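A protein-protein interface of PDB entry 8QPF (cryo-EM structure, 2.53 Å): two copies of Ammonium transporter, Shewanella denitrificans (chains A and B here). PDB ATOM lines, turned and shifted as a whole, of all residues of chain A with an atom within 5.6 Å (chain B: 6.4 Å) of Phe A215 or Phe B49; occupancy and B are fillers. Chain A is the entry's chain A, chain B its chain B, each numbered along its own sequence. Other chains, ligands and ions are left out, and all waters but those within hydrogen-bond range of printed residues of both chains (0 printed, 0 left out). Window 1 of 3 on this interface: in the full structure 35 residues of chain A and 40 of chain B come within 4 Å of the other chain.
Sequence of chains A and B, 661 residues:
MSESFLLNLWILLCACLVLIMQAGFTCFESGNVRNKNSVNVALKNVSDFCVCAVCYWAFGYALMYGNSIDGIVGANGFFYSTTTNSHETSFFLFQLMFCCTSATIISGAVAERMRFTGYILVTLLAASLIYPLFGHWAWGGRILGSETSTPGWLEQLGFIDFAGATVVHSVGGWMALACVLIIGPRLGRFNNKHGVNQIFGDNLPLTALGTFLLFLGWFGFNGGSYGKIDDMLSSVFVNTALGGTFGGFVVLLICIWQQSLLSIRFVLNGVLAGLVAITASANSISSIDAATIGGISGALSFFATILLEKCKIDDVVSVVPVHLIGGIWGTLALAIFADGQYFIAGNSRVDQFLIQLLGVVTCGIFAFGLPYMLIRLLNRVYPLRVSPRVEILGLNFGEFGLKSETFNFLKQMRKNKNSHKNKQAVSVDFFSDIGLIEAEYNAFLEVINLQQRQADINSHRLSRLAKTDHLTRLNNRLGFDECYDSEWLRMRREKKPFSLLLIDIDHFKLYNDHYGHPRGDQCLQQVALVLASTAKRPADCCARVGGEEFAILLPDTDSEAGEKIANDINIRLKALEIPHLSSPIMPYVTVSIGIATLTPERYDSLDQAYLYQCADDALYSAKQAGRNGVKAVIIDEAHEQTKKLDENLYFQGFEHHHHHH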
ATOM      1  N   GLY A 210     -11.193   5.107  26.780  1.00  0.00           N
ATOM      2  CA  GLY A 210     -11.228   5.133  28.231  1.00  0.00           C
ATOM      3  C   GLY A 210     -10.893   3.794  28.857  1.00  0.00           C
ATOM      4  O   GLY A 210     -10.232   3.737  29.892  1.00  0.00           O
ATOM      5  N   THR A 211     -11.324   2.700  28.223  1.00  0.00           N
ATOM      6  CA  THR A 211     -10.989   1.364  28.711  1.00  0.00           C
ATOM      7  C   THR A 211      -9.494   1.081  28.585  1.00  0.00           C
ATOM      8  O   THR A 211      -8.889   0.482  29.486  1.00  0.00           O
ATOM      9  CB  THR A 211     -11.803   0.319  27.949  1.00  0.00           C
ATOM     10  OG1 THR A 211     -13.191   0.675  27.989  1.00  0.00           O
ATOM     11  CG2 THR A 211     -11.635  -1.061  28.563  1.00  0.00           C
ATOM     12  N   PHE A 212      -8.880   1.517  27.478  1.00  0.00           N
ATOM     13  CA  PHE A 212      -7.432   1.370  27.330  1.00  0.00           C
ATOM     14  C   PHE A 212      -6.669   2.202  28.362  1.00  0.00           C
ATOM     15  O   PHE A 212      -5.670   1.738  28.936  1.00  0.00           O
ATOM     16  CB  PHE A 212      -7.008   1.752  25.914  1.00  0.00           C
ATOM     17  CG  PHE A 212      -6.904   0.585  24.978  1.00  0.00           C
ATOM     18  CD1 PHE A 212      -5.994  -0.432  25.220  1.00  0.00           C
ATOM     19  CD2 PHE A 212      -7.713   0.504  23.856  1.00  0.00           C
ATOM     20  CE1 PHE A 212      -5.896  -1.511  24.363  1.00  0.00           C
ATOM     21  CE2 PHE A 212      -7.618  -0.573  22.993  1.00  0.00           C
ATOM     22  CZ  PHE A 212      -6.708  -1.580  23.247  1.00  0.00           C
ATOM     23  N   LEU A 213      -7.139   3.427  28.628  1.00  0.00           N
ATOM     24  CA  LEU A 213      -6.518   4.259  29.657  1.00  0.00           C
ATOM     25  C   LEU A 213      -6.714   3.666  31.050  1.00  0.00           C
ATOM     26  O   LEU A 213      -5.845   3.804  31.919  1.00  0.00           O
ATOM     27  CB  LEU A 213      -7.083   5.678  29.595  1.00  0.00           C
ATOM     28  CG  LEU A 213      -6.724   6.545  28.386  1.00  0.00           C
ATOM     29  CD1 LEU A 213      -7.283   7.945  28.555  1.00  0.00           C
ATOM     30  CD2 LEU A 213      -5.225   6.592  28.169  1.00  0.00           C
ATOM     31  N   LEU A 214      -7.844   2.991  31.275  1.00  0.00           N
ATOM     32  CA  LEU A 214      -8.082   2.322  32.551  1.00  0.00           C
ATOM     33  C   LEU A 214      -7.163   1.121  32.738  1.00  0.00           C
ATOM     34  O   LEU A 214      -6.682   0.880  33.849  1.00  0.00           O
ATOM     35  CB  LEU A 214      -9.544   1.899  32.653  1.00  0.00           C
ATOM     36  CG  LEU A 214     -10.500   3.015  33.064  1.00  0.00           C
ATOM     37  CD1 LEU A 214     -11.933   2.694  32.668  1.00  0.00           C
ATOM     38  CD2 LEU A 214     -10.376   3.257  34.536  1.00  0.00           C
ATOM     39  N   PHE A 215      -6.916   0.360  31.665  1.00  0.00           N
ATOM     40  CA  PHE A 215      -5.927  -0.721  31.693  1.00  0.00           C
ATOM     41  C   PHE A 215      -4.540  -0.187  32.044  1.00  0.00           C
ATOM     42  O   PHE A 215      -3.834  -0.739  32.912  1.00  0.00           O
ATOM     43  CB  PHE A 215      -5.903  -1.408  30.323  1.00  0.00           C
ATOM     44  CG  PHE A 215      -5.624  -2.889  30.363  1.00  0.00           C
ATOM     45  CD1 PHE A 215      -4.627  -3.415  31.170  1.00  0.00           C
ATOM     46  CD2 PHE A 215      -6.353  -3.754  29.562  1.00  0.00           C
ATOM     47  CE1 PHE A 215      -4.374  -4.769  31.191  1.00  0.00           C
ATOM     48  CE2 PHE A 215      -6.105  -5.113  29.580  1.00  0.00           C
ATOM     49  CZ  PHE A 215      -5.113  -5.619  30.394  1.00  0.00           C
ATOM     50  N   LEU A 216      -4.159   0.912  31.387  1.00  0.00           N
ATOM     51  CA  LEU A 216      -2.863   1.538  31.616  1.00  0.00           C
ATOM     52  C   LEU A 216      -2.705   2.011  33.054  1.00  0.00           C
ATOM     53  O   LEU A 216      -1.699   1.721  33.713  1.00  0.00           O
ATOM     54  CB  LEU A 216      -2.702   2.709  30.661  1.00  0.00           C
ATOM     55  CG  LEU A 216      -1.387   3.388  30.969  1.00  0.00           C
ATOM     56  CD1 LEU A 216      -0.288   2.603  30.376  1.00  0.00           C
ATOM     57  CD2 LEU A 216      -1.410   4.757  30.472  1.00  0.00           C
ATOM     58  N   GLY A 217      -3.711   2.709  33.575  1.00  0.00           N
ATOM     59  CA  GLY A 217      -3.649   3.129  34.955  1.00  0.00           C
ATOM     60  C   GLY A 217      -3.803   2.005  35.949  1.00  0.00           C
ATOM     61  O   GLY A 217      -3.420   2.159  37.113  1.00  0.00           O
ATOM     62  N   TRP A 218      -4.346   0.873  35.511  1.00  0.00           N
ATOM     63  CA  TRP A 218      -4.521  -0.246  36.412  1.00  0.00           C
ATOM     64  C   TRP A 218      -3.185  -0.922  36.659  1.00  0.00           C
ATOM     65  O   TRP A 218      -2.953  -1.504  37.732  1.00  0.00           O
ATOM     66  CB  TRP A 218      -5.468  -1.246  35.780  1.00  0.00           C
ATOM     67  CG  TRP A 218      -6.215  -1.933  36.774  1.00  0.00           C
ATOM     68  CD1 TRP A 218      -5.821  -2.928  37.607  1.00  0.00           C
ATOM     69  CD2 TRP A 218      -7.578  -1.684  37.042  1.00  0.00           C
ATOM     70  NE1 TRP A 218      -6.874  -3.295  38.411  1.00  0.00           N
ATOM     71  CE2 TRP A 218      -7.967  -2.541  38.071  1.00  0.00           C
ATOM     72  CE3 TRP A 218      -8.517  -0.804  36.499  1.00  0.00           C
ATOM     73  CZ2 TRP A 218      -9.254  -2.546  38.569  1.00  0.00           C
ATOM     74  CZ3 TRP A 218      -9.785  -0.811  36.991  1.00  0.00           C
ATOM     75  CH2 TRP A 218     -10.143  -1.671  38.009  1.00  0.00           C
ATOM     76  N   PHE A 219      -2.320  -0.871  35.640  1.00  0.00           N
ATOM     77  CA  PHE A 219      -0.919  -1.250  35.819  1.00  0.00           C
ATOM     78  C   PHE A 219      -0.267  -0.451  36.945  1.00  0.00           C
ATOM     79  O   PHE A 219       0.414  -1.015  37.807  1.00  0.00           O
ATOM     80  CB  PHE A 219      -0.150  -1.043  34.516  1.00  0.00           C
ATOM     81  CG  PHE A 219      -0.275  -2.178  33.558  1.00  0.00           C
ATOM     82  CD1 PHE A 219       0.262  -3.412  33.861  1.00  0.00           C
ATOM     83  CD2 PHE A 219      -0.926  -2.013  32.348  1.00  0.00           C
ATOM     84  CE1 PHE A 219       0.152  -4.456  32.979  1.00  0.00           C
ATOM     85  CE2 PHE A 219      -1.039  -3.064  31.466  1.00  0.00           C
ATOM     86  CZ  PHE A 219      -0.498  -4.285  31.783  1.00  0.00           C
ATOM     87  N   GLY A 220      -0.489   0.866  36.961  1.00  0.00           N
ATOM     88  CA  GLY A 220       0.062   1.697  38.021  1.00  0.00           C
ATOM     89  C   GLY A 220      -0.577   1.460  39.376  1.00  0.00           C
ATOM     90  O   GLY A 220       0.099   1.544  40.403  1.00  0.00           O
ATOM     91  N   THR A 240      -1.738  -8.510  35.839  1.00  0.00           N
ATOM     92  CA  THR A 240      -2.670  -7.439  35.483  1.00  0.00           C
ATOM     93  C   THR A 240      -3.085  -7.516  34.016  1.00  0.00           C
ATOM     94  O   THR A 240      -4.288  -7.481  33.689  1.00  0.00           O
ATOM     95  CB  THR A 240      -2.038  -6.081  35.790  1.00  0.00           C
ATOM     96  OG1 THR A 240      -1.423  -6.121  37.082  1.00  0.00           O
ATOM     97  CG2 THR A 240      -3.081  -4.978  35.765  1.00  0.00           C
ATOM     98  N   ALA A 241      -2.093  -7.655  33.128  1.00  0.00           N
ATOM     99  CA  ALA A 241      -2.360  -7.750  31.696  1.00  0.00           C
ATOM    100  C   ALA A 241      -3.185  -8.987  31.360  1.00  0.00           C
ATOM    101  O   ALA A 241      -4.146  -8.907  30.586  1.00  0.00           O
ATOM    102  CB  ALA A 241      -1.046  -7.760  30.919  1.00  0.00           C
ATOM    103  N   LEU A 242      -2.851 -10.127  31.972  1.00  0.00           N
ATOM    104  CA  LEU A 242      -3.551 -11.366  31.658  1.00  0.00           C
ATOM    105  C   LEU A 242      -4.974 -11.365  32.196  1.00  0.00           C
ATOM    106  O   LEU A 242      -5.880 -11.873  31.529  1.00  0.00           O
ATOM    107  CB  LEU A 242      -2.767 -12.561  32.191  1.00  0.00           C
ATOM    108  CG  LEU A 242      -1.526 -12.878  31.358  1.00  0.00           C
ATOM    109  CD1 LEU A 242      -0.823 -14.072  31.929  1.00  0.00           C
ATOM    110  CD2 LEU A 242      -1.883 -13.113  29.901  1.00  0.00           C
ATOM    111  N   GLY A 243      -5.198 -10.768  33.374  1.00  0.00           N
ATOM    112  CA  GLY A 243      -6.553 -10.670  33.899  1.00  0.00           C
ATOM    113  C   GLY A 243      -7.458  -9.813  33.034  1.00  0.00           C
ATOM    114  O   GLY A 243      -8.571 -10.230  32.679  1.00  0.00           O
ATOM    115  N   GLY A 244      -6.969  -8.632  32.630  1.00  0.00           N
ATOM    116  CA  GLY A 244      -7.776  -7.767  31.774  1.00  0.00           C
ATOM    117  C   GLY A 244      -8.044  -8.364  30.402  1.00  0.00           C
ATOM    118  O   GLY A 244      -9.189  -8.375  29.920  1.00  0.00           O
ATOM    119  N   THR A 245      -7.000  -8.917  29.773  1.00  0.00           N
ATOM    120  CA  THR A 245      -7.156  -9.442  28.422  1.00  0.00           C
ATOM    121  C   THR A 245      -7.959 -10.736  28.406  1.00  0.00           C
ATOM    122  O   THR A 245      -8.693 -10.993  27.449  1.00  0.00           O
ATOM    123  CB  THR A 245      -5.790  -9.645  27.772  1.00  0.00           C
ATOM    124  OG1 THR A 245      -4.954 -10.424  28.635  1.00  0.00           O
ATOM    125  CG2 THR A 245      -5.143  -8.300  27.518  1.00  0.00           C
ATOM    126  N   VAL A 271     -13.220  -6.577  30.216  1.00  0.00           N
ATOM    127  CA  VAL A 271     -11.836  -6.145  30.447  1.00  0.00           C
ATOM    128  C   VAL A 271     -11.697  -5.510  31.826  1.00  0.00           C
ATOM    129  O   VAL A 271     -10.829  -5.889  32.632  1.00  0.00           O
ATOM    130  CB  VAL A 271     -11.388  -5.157  29.351  1.00  0.00           C
ATOM    131  CG1 VAL A 271     -10.051  -4.524  29.710  1.00  0.00           C
ATOM    132  CG2 VAL A 271     -11.297  -5.823  28.006  1.00  0.00           C
ATOM    133  N   LEU A 272     -12.589  -4.559  32.127  1.00  0.00           N
ATOM    134  CA  LEU A 272     -12.510  -3.836  33.392  1.00  0.00           C
ATOM    135  C   LEU A 272     -12.805  -4.743  34.582  1.00  0.00           C
ATOM    136  O   LEU A 272     -12.151  -4.631  35.620  1.00  0.00           O
ATOM    137  CB  LEU A 272     -13.456  -2.638  33.371  1.00  0.00           C
ATOM    138  CG  LEU A 272     -13.195  -1.571  32.309  1.00  0.00           C
ATOM    139  CD1 LEU A 272     -14.166  -0.414  32.462  1.00  0.00           C
ATOM    140  CD2 LEU A 272     -11.756  -1.090  32.364  1.00  0.00           C
ATOM    141  N   LEU A 275      -9.853  -6.862  35.362  1.00  0.00           N
ATOM    142  CA  LEU A 275      -8.904  -6.030  36.106  1.00  0.00           C
ATOM    143  C   LEU A 275      -9.308  -5.868  37.577  1.00  0.00           C
ATOM    144  O   LEU A 275      -8.453  -5.946  38.474  1.00  0.00           O
ATOM    145  CB  LEU A 275      -8.769  -4.672  35.421  1.00  0.00           C
ATOM    146  CG  LEU A 275      -8.030  -4.674  34.081  1.00  0.00           C
ATOM    147  CD1 LEU A 275      -8.239  -3.364  33.341  1.00  0.00           C
ATOM    148  CD2 LEU A 275      -6.552  -4.944  34.277  1.00  0.00           C
ATOM    149  N   LEU B  19       1.162   0.070  25.563  1.00  0.00           N
ATOM    150  CA  LEU B  19      -0.294   0.047  25.763  1.00  0.00           C
ATOM    151  C   LEU B  19      -0.940   1.386  25.392  1.00  0.00           C
ATOM    152  O   LEU B  19      -2.054   1.427  24.836  1.00  0.00           O
ATOM    153  CB  LEU B  19      -0.630  -0.333  27.203  1.00  0.00           C
ATOM    154  CG  LEU B  19      -2.115  -0.602  27.461  1.00  0.00           C
ATOM    155  CD1 LEU B  19      -2.637  -1.708  26.566  1.00  0.00           C
ATOM    156  CD2 LEU B  19      -2.349  -0.950  28.903  1.00  0.00           C
ATOM    157  N   GLN B  22      -1.362   1.301  21.797  1.00  0.00           N
ATOM    158  CA  GLN B  22      -2.610   0.616  21.435  1.00  0.00           C
ATOM    159  C   GLN B  22      -3.811   1.555  21.508  1.00  0.00           C
ATOM    160  O   GLN B  22      -4.685   1.532  20.627  1.00  0.00           O
ATOM    161  CB  GLN B  22      -2.854  -0.591  22.342  1.00  0.00           C
ATOM    162  CG  GLN B  22      -1.712  -1.557  22.414  1.00  0.00           C
ATOM    163  CD  GLN B  22      -1.450  -2.235  21.099  1.00  0.00           C
ATOM    164  OE1 GLN B  22      -0.331  -2.212  20.597  1.00  0.00           O
ATOM    165  NE2 GLN B  22      -2.478  -2.858  20.535  1.00  0.00           N
ATOM    166  N   LYS B  44     -13.085  -3.874  17.161  1.00  0.00           N
ATOM    167  CA  LYS B  44     -11.968  -4.596  16.555  1.00  0.00           C
ATOM    168  C   LYS B  44     -10.652  -4.272  17.250  1.00  0.00           C
ATOM    169  O   LYS B  44      -9.847  -5.171  17.519  1.00  0.00           O
ATOM    170  CB  LYS B  44     -11.873  -4.251  15.068  1.00  0.00           C
ATOM    171  CG  LYS B  44     -12.784  -5.065  14.167  1.00  0.00           C
ATOM    172  CD  LYS B  44     -12.911  -4.470  12.764  1.00  0.00           C
ATOM    173  CE  LYS B  44     -11.577  -3.992  12.209  1.00  0.00           C
ATOM    174  NZ  LYS B  44     -11.749  -2.940  11.172  1.00  0.00           N
ATOM    175  N   ASN B  45     -10.436  -2.994  17.573  1.00  0.00           N
ATOM    176  CA  ASN B  45      -9.178  -2.554  18.168  1.00  0.00           C
ATOM    177  C   ASN B  45      -9.011  -3.040  19.602  1.00  0.00           C
ATOM    178  O   ASN B  45      -7.883  -3.116  20.099  1.00  0.00           O
ATOM    179  CB  ASN B  45      -9.088  -1.030  18.120  1.00  0.00           C
ATOM    180  CG  ASN B  45      -8.466  -0.524  16.839  1.00  0.00           C
ATOM    181  OD1 ASN B  45      -8.920   0.465  16.266  1.00  0.00           O
ATOM    182  ND2 ASN B  45      -7.417  -1.193  16.386  1.00  0.00           N
ATOM    183  N   VAL B  46     -10.107  -3.347  20.288  1.00  0.00           N
ATOM    184  CA  VAL B  46      -9.994  -3.961  21.612  1.00  0.00           C
ATOM    185  C   VAL B  46      -9.888  -5.484  21.519  1.00  0.00           C
ATOM    186  O   VAL B  46      -9.074  -6.108  22.220  1.00  0.00           O
ATOM    187  CB  VAL B  46     -11.183  -3.515  22.486  1.00  0.00           C
ATOM    188  CG1 VAL B  46     -11.159  -4.200  23.844  1.00  0.00           C
ATOM    189  CG2 VAL B  46     -11.154  -2.009  22.659  1.00  0.00           C
ATOM    190  N   SER B  47     -10.689  -6.085  20.631  1.00  0.00           N
ATOM    191  CA  SER B  47     -10.757  -7.537  20.522  1.00  0.00           C
ATOM    192  C   SER B  47      -9.456  -8.128  19.999  1.00  0.00           C
ATOM    193  O   SER B  47      -9.031  -9.191  20.465  1.00  0.00           O
ATOM    194  CB  SER B  47     -11.926  -7.932  19.623  1.00  0.00           C
ATOM    195  OG  SER B  47     -13.108  -7.260  20.013  1.00  0.00           O
ATOM    196  N   ASP B  48      -8.802  -7.458  19.041  1.00  0.00           N
ATOM    197  CA  ASP B  48      -7.542  -7.987  18.528  1.00  0.00           C
ATOM    198  C   ASP B  48      -6.430  -7.897  19.565  1.00  0.00           C
ATOM    199  O   ASP B  48      -5.561  -8.770  19.620  1.00  0.00           O
ATOM    200  CB  ASP B  48      -7.159  -7.306  17.204  1.00  0.00           C
ATOM    201  CG  ASP B  48      -6.823  -5.804  17.326  1.00  0.00           C
ATOM    202  OD1 ASP B  48      -6.813  -5.201  18.418  1.00  0.00           O
ATOM    203  OD2 ASP B  48      -6.556  -5.204  16.265  1.00  0.00           O
ATOM    204  N   PHE B  49      -6.456  -6.854  20.401  1.00  0.00           N
ATOM    205  CA  PHE B  49      -5.504  -6.739  21.502  1.00  0.00           C
ATOM    206  C   PHE B  49      -5.671  -7.881  22.496  1.00  0.00           C
ATOM    207  O   PHE B  49      -4.683  -8.504  22.913  1.00  0.00           O
ATOM    208  CB  PHE B  49      -5.677  -5.387  22.197  1.00  0.00           C
ATOM    209  CG  PHE B  49      -4.993  -5.298  23.529  1.00  0.00           C
ATOM    210  CD1 PHE B  49      -3.613  -5.351  23.623  1.00  0.00           C
ATOM    211  CD2 PHE B  49      -5.735  -5.158  24.690  1.00  0.00           C
ATOM    212  CE1 PHE B  49      -2.983  -5.276  24.849  1.00  0.00           C
ATOM    213  CE2 PHE B  49      -5.112  -5.075  25.920  1.00  0.00           C
ATOM    214  CZ  PHE B  49      -3.734  -5.137  26.000  1.00  0.00           C
ATOM    215  N   CYS B  50      -6.923  -8.193  22.854  1.00  0.00           N
ATOM    216  CA  CYS B  50      -7.178  -9.299  23.780  1.00  0.00           C
ATOM    217  C   CYS B  50      -6.776 -10.645  23.176  1.00  0.00           C
ATOM    218  O   CYS B  50      -6.133 -11.470  23.841  1.00  0.00           O
ATOM    219  CB  CYS B  50      -8.649  -9.307  24.194  1.00  0.00           C
ATOM    220  SG  CYS B  50      -9.158  -7.874  25.166  1.00  0.00           S
ATOM    221  N   VAL B  51      -7.115 -10.864  21.899  1.00  0.00           N
ATOM    222  CA  VAL B  51      -6.816 -12.131  21.230  1.00  0.00           C
ATOM    223  C   VAL B  51      -5.310 -12.315  21.061  1.00  0.00           C
ATOM    224  O   VAL B  51      -4.775 -13.407  21.296  1.00  0.00           O
ATOM    225  CB  VAL B  51      -7.570 -12.205  19.884  1.00  0.00           C
ATOM    226  CG1 VAL B  51      -7.005 -13.287  18.972  1.00  0.00           C
ATOM    227  CG2 VAL B  51      -9.045 -12.464  20.125  1.00  0.00           C
ATOM    228  N   CYS B  52      -4.595 -11.243  20.702  1.00  0.00           N
ATOM    229  CA  CYS B  52      -3.147 -11.320  20.537  1.00  0.00           C
ATOM    230  C   CYS B  52      -2.433 -11.531  21.861  1.00  0.00           C
ATOM    231  O   CYS B  52      -1.429 -12.248  21.909  1.00  0.00           O
ATOM    232  CB  CYS B  52      -2.623 -10.058  19.864  1.00  0.00           C
ATOM    233  SG  CYS B  52      -2.977  -9.996  18.133  1.00  0.00           S
ATOM    234  N   ALA B  53      -2.922 -10.910  22.939  1.00  0.00           N
ATOM    235  CA  ALA B  53      -2.323 -11.138  24.251  1.00  0.00           C
ATOM    236  C   ALA B  53      -2.512 -12.582  24.704  1.00  0.00           C
ATOM    237  O   ALA B  53      -1.572 -13.208  25.213  1.00  0.00           O
ATOM    238  CB  ALA B  53      -2.913 -10.168  25.268  1.00  0.00           C
ATOM    239  N   VAL B  54      -3.715 -13.134  24.490  1.00  0.00           N
ATOM    240  CA  VAL B  54      -3.982 -14.535  24.831  1.00  0.00           C
ATOM    241  C   VAL B  54      -3.113 -15.473  23.995  1.00  0.00           C
ATOM    242  O   VAL B  54      -2.521 -16.428  24.520  1.00  0.00           O
ATOM    243  CB  VAL B  54      -5.486 -14.840  24.667  1.00  0.00           C
ATOM    244  CG1 VAL B  54      -5.762 -16.333  24.722  1.00  0.00           C
ATOM    245  CG2 VAL B  54      -6.289 -14.134  25.744  1.00  0.00           C
ATOM    246  N   LEU B  96       4.909  -9.156  24.160  1.00  0.00           N
ATOM    247  CA  LEU B  96       3.470  -9.335  24.008  1.00  0.00           C
ATOM    248  C   LEU B  96       2.812  -8.066  23.491  1.00  0.00           C
ATOM    249  O   LEU B  96       1.926  -8.121  22.625  1.00  0.00           O
ATOM    250  CB  LEU B  96       2.859  -9.764  25.343  1.00  0.00           C
ATOM    251  CG  LEU B  96       1.358 -10.050  25.419  1.00  0.00           C
ATOM    252  CD1 LEU B  96       1.119 -11.354  26.150  1.00  0.00           C
ATOM    253  CD2 LEU B  96       0.620  -8.918  26.119  1.00  0.00           C
ATOM    254  N   MET B  97       3.246  -6.910  23.995  1.00  0.00           N
ATOM    255  CA  MET B  97       2.686  -5.659  23.495  1.00  0.00           C
ATOM    256  C   MET B  97       3.132  -5.378  22.061  1.00  0.00           C
ATOM    257  O   MET B  97       2.381  -4.785  21.277  1.00  0.00           O
ATOM    258  CB  MET B  97       3.053  -4.498  24.424  1.00  0.00           C
ATOM    259  CG  MET B  97       2.587  -4.654  25.872  1.00  0.00           C
ATOM    260  SD  MET B  97       0.857  -4.380  26.326  1.00  0.00           S
ATOM    261  CE  MET B  97       0.188  -3.494  24.928  1.00  0.00           C
ATOM    262  N   CYS B 100       0.783  -7.464  19.956  1.00  0.00           N
ATOM    263  CA  CYS B 100      -0.506  -6.784  19.849  1.00  0.00           C
ATOM    264  C   CYS B 100      -0.429  -5.600  18.890  1.00  0.00           C
ATOM    265  O   CYS B 100      -1.397  -5.308  18.168  1.00  0.00           O
ATOM    266  CB  CYS B 100      -0.974  -6.337  21.231  1.00  0.00           C
ATOM    267  SG  CYS B 100      -1.280  -7.702  22.370  1.00  0.00           S
ATOM    268  N   THR B 104      -2.833  -4.774  15.580  1.00  0.00           N
ATOM    269  CA  THR B 104      -3.598  -3.534  15.594  1.00  0.00           C
ATOM    270  C   THR B 104      -3.128  -2.576  14.498  1.00  0.00           C
ATOM    271  O   THR B 104      -3.860  -1.646  14.145  1.00  0.00           O
ATOM    272  CB  THR B 104      -3.560  -2.894  16.983  1.00  0.00           C
ATOM    273  OG1 THR B 104      -4.672  -2.002  17.128  1.00  0.00           O
ATOM    274  CG2 THR B 104      -2.297  -2.139  17.199  1.00  0.00           C
ATOM    275  N   TYR B 119     -11.999 -10.852  10.596  1.00  0.00           N
ATOM    276  CA  TYR B 119     -10.877 -10.089  11.129  1.00  0.00           C
ATOM    277  C   TYR B 119     -10.280 -10.775  12.356  1.00  0.00           C
ATOM    278  O   TYR B 119      -9.062 -10.739  12.561  1.00  0.00           O
ATOM    279  CB  TYR B 119     -11.292  -8.652  11.468  1.00  0.00           C
ATOM    280  CG  TYR B 119     -10.177  -7.950  12.198  1.00  0.00           C
ATOM    281  CD1 TYR B 119      -8.981  -7.680  11.545  1.00  0.00           C
ATOM    282  CD2 TYR B 119     -10.278  -7.632  13.548  1.00  0.00           C
ATOM    283  CE1 TYR B 119      -7.934  -7.087  12.197  1.00  0.00           C
ATOM    284  CE2 TYR B 119      -9.230  -7.034  14.212  1.00  0.00           C
ATOM    285  CZ  TYR B 119      -8.064  -6.764  13.525  1.00  0.00           C
ATOM    286  OH  TYR B 119      -7.004  -6.183  14.164  1.00  0.00           O
ATOM    287  N   THR B 123      -6.471 -11.927  12.722  1.00  0.00           N
ATOM    288  CA  THR B 123      -5.685 -11.585  13.907  1.00  0.00           C
ATOM    289  C   THR B 123      -5.101 -12.836  14.565  1.00  0.00           C
ATOM    290  O   THR B 123      -3.949 -12.826  15.021  1.00  0.00           O
ATOM    291  CB  THR B 123      -6.575 -10.785  14.871  1.00  0.00           C
ATOM    292  OG1 THR B 123      -6.639  -9.425  14.433  1.00  0.00           O
ATOM    293  CG2 THR B 123      -6.071 -10.810  16.307  1.00  0.00           C
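No position is printed for both chains. Of the 12 pairs that touch across the chains among the printed residues, none has its exchanged pair printed and touching as well.
Hydrophobic or aromatic side chains of chain A within 4 Å of the printed part of chain B: Phe A212, Phe A215 and Phe A219. Among the printed residues, no Asp or Glu carboxylate lies within 4 Å of a Lys or Arg side-chain nitrogen of the other chain.
O of Leu A242 is in hydrogen-bond range of OG1 of Thr A245 (3.4 Å). The side-chain sulfur of Cys B50 lies within hydrogen-bond range of the backbone carbonyl oxygen of Val B46, at 3.4 Å. The side-chain sulfur of Cys B100 lies within hydrogen-bond range of the backbone carbonyl oxygen of Phe B49. ND2 of Asn B45 sits at hydrogen-bond distance from OG1 of Thr B104, at 3.0 Å. N of Ala B53 sits at hydrogen-bond distance from SG of Cys B100, at 3.6 Å. The backbone carbonyl oxygen (O) of Ala A241 lies within hydrogen-bond range of the side-chain hydroxyl (OG1) of Thr A245 (2.6 Å).
Of chain B, only Leu B19 (3.9 Å) and Phe B49 (3.8 Å) come within 4 Å of Phe A215. Of chain A, only Phe A212, Phe A215 and Thr A245 come within 4 Å of Phe B49. Printed residues of chain B within 4 Å of Thr A245: Phe B49 (3.6 Å), Cys B50 (3.7 Å) and Ala B53 (3.7 Å). Of the printed residues of chain B, Phe A212 touches Leu B19, Gln B22, Asn B45, Val B46 and Phe B49. Of the printed residues of chain A, Leu B19 touches Phe A212, Phe A215, Leu A216 and Phe A219. Printed residues of chain A within 4 Å of Gln B22: Phe A212. The nearest printed residue of chain A that does not touch Phe B49 is Ala A241 (6.0 Å). The nearest printed residue of chain B that does not touch Thr A245 is Val B54 (4.3 Å).
Among the printed residues, merely in contact across the chains: Phe A219 with Leu B19 (3.6 Å), Leu A216 with Leu B19 (3.6 Å), Thr A245 with Phe B49 (3.6 Å), Phe A212 with Phe B49 (3.7 Å), Thr A245 with Cys B50 (3.7 Å), Thr A245 with Ala B53 (3.7 Å), Phe A212 with Asn B45 (3.7 Å), Phe A212 with Gln B22 (3.8 Å), Phe A215 with Phe B49 (3.8 Å), Phe A212 with Val B46 (3.8 Å), Phe A212 with Leu B19 (3.8 Å) and Phe A215 with Leu B19 (3.9 Å).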
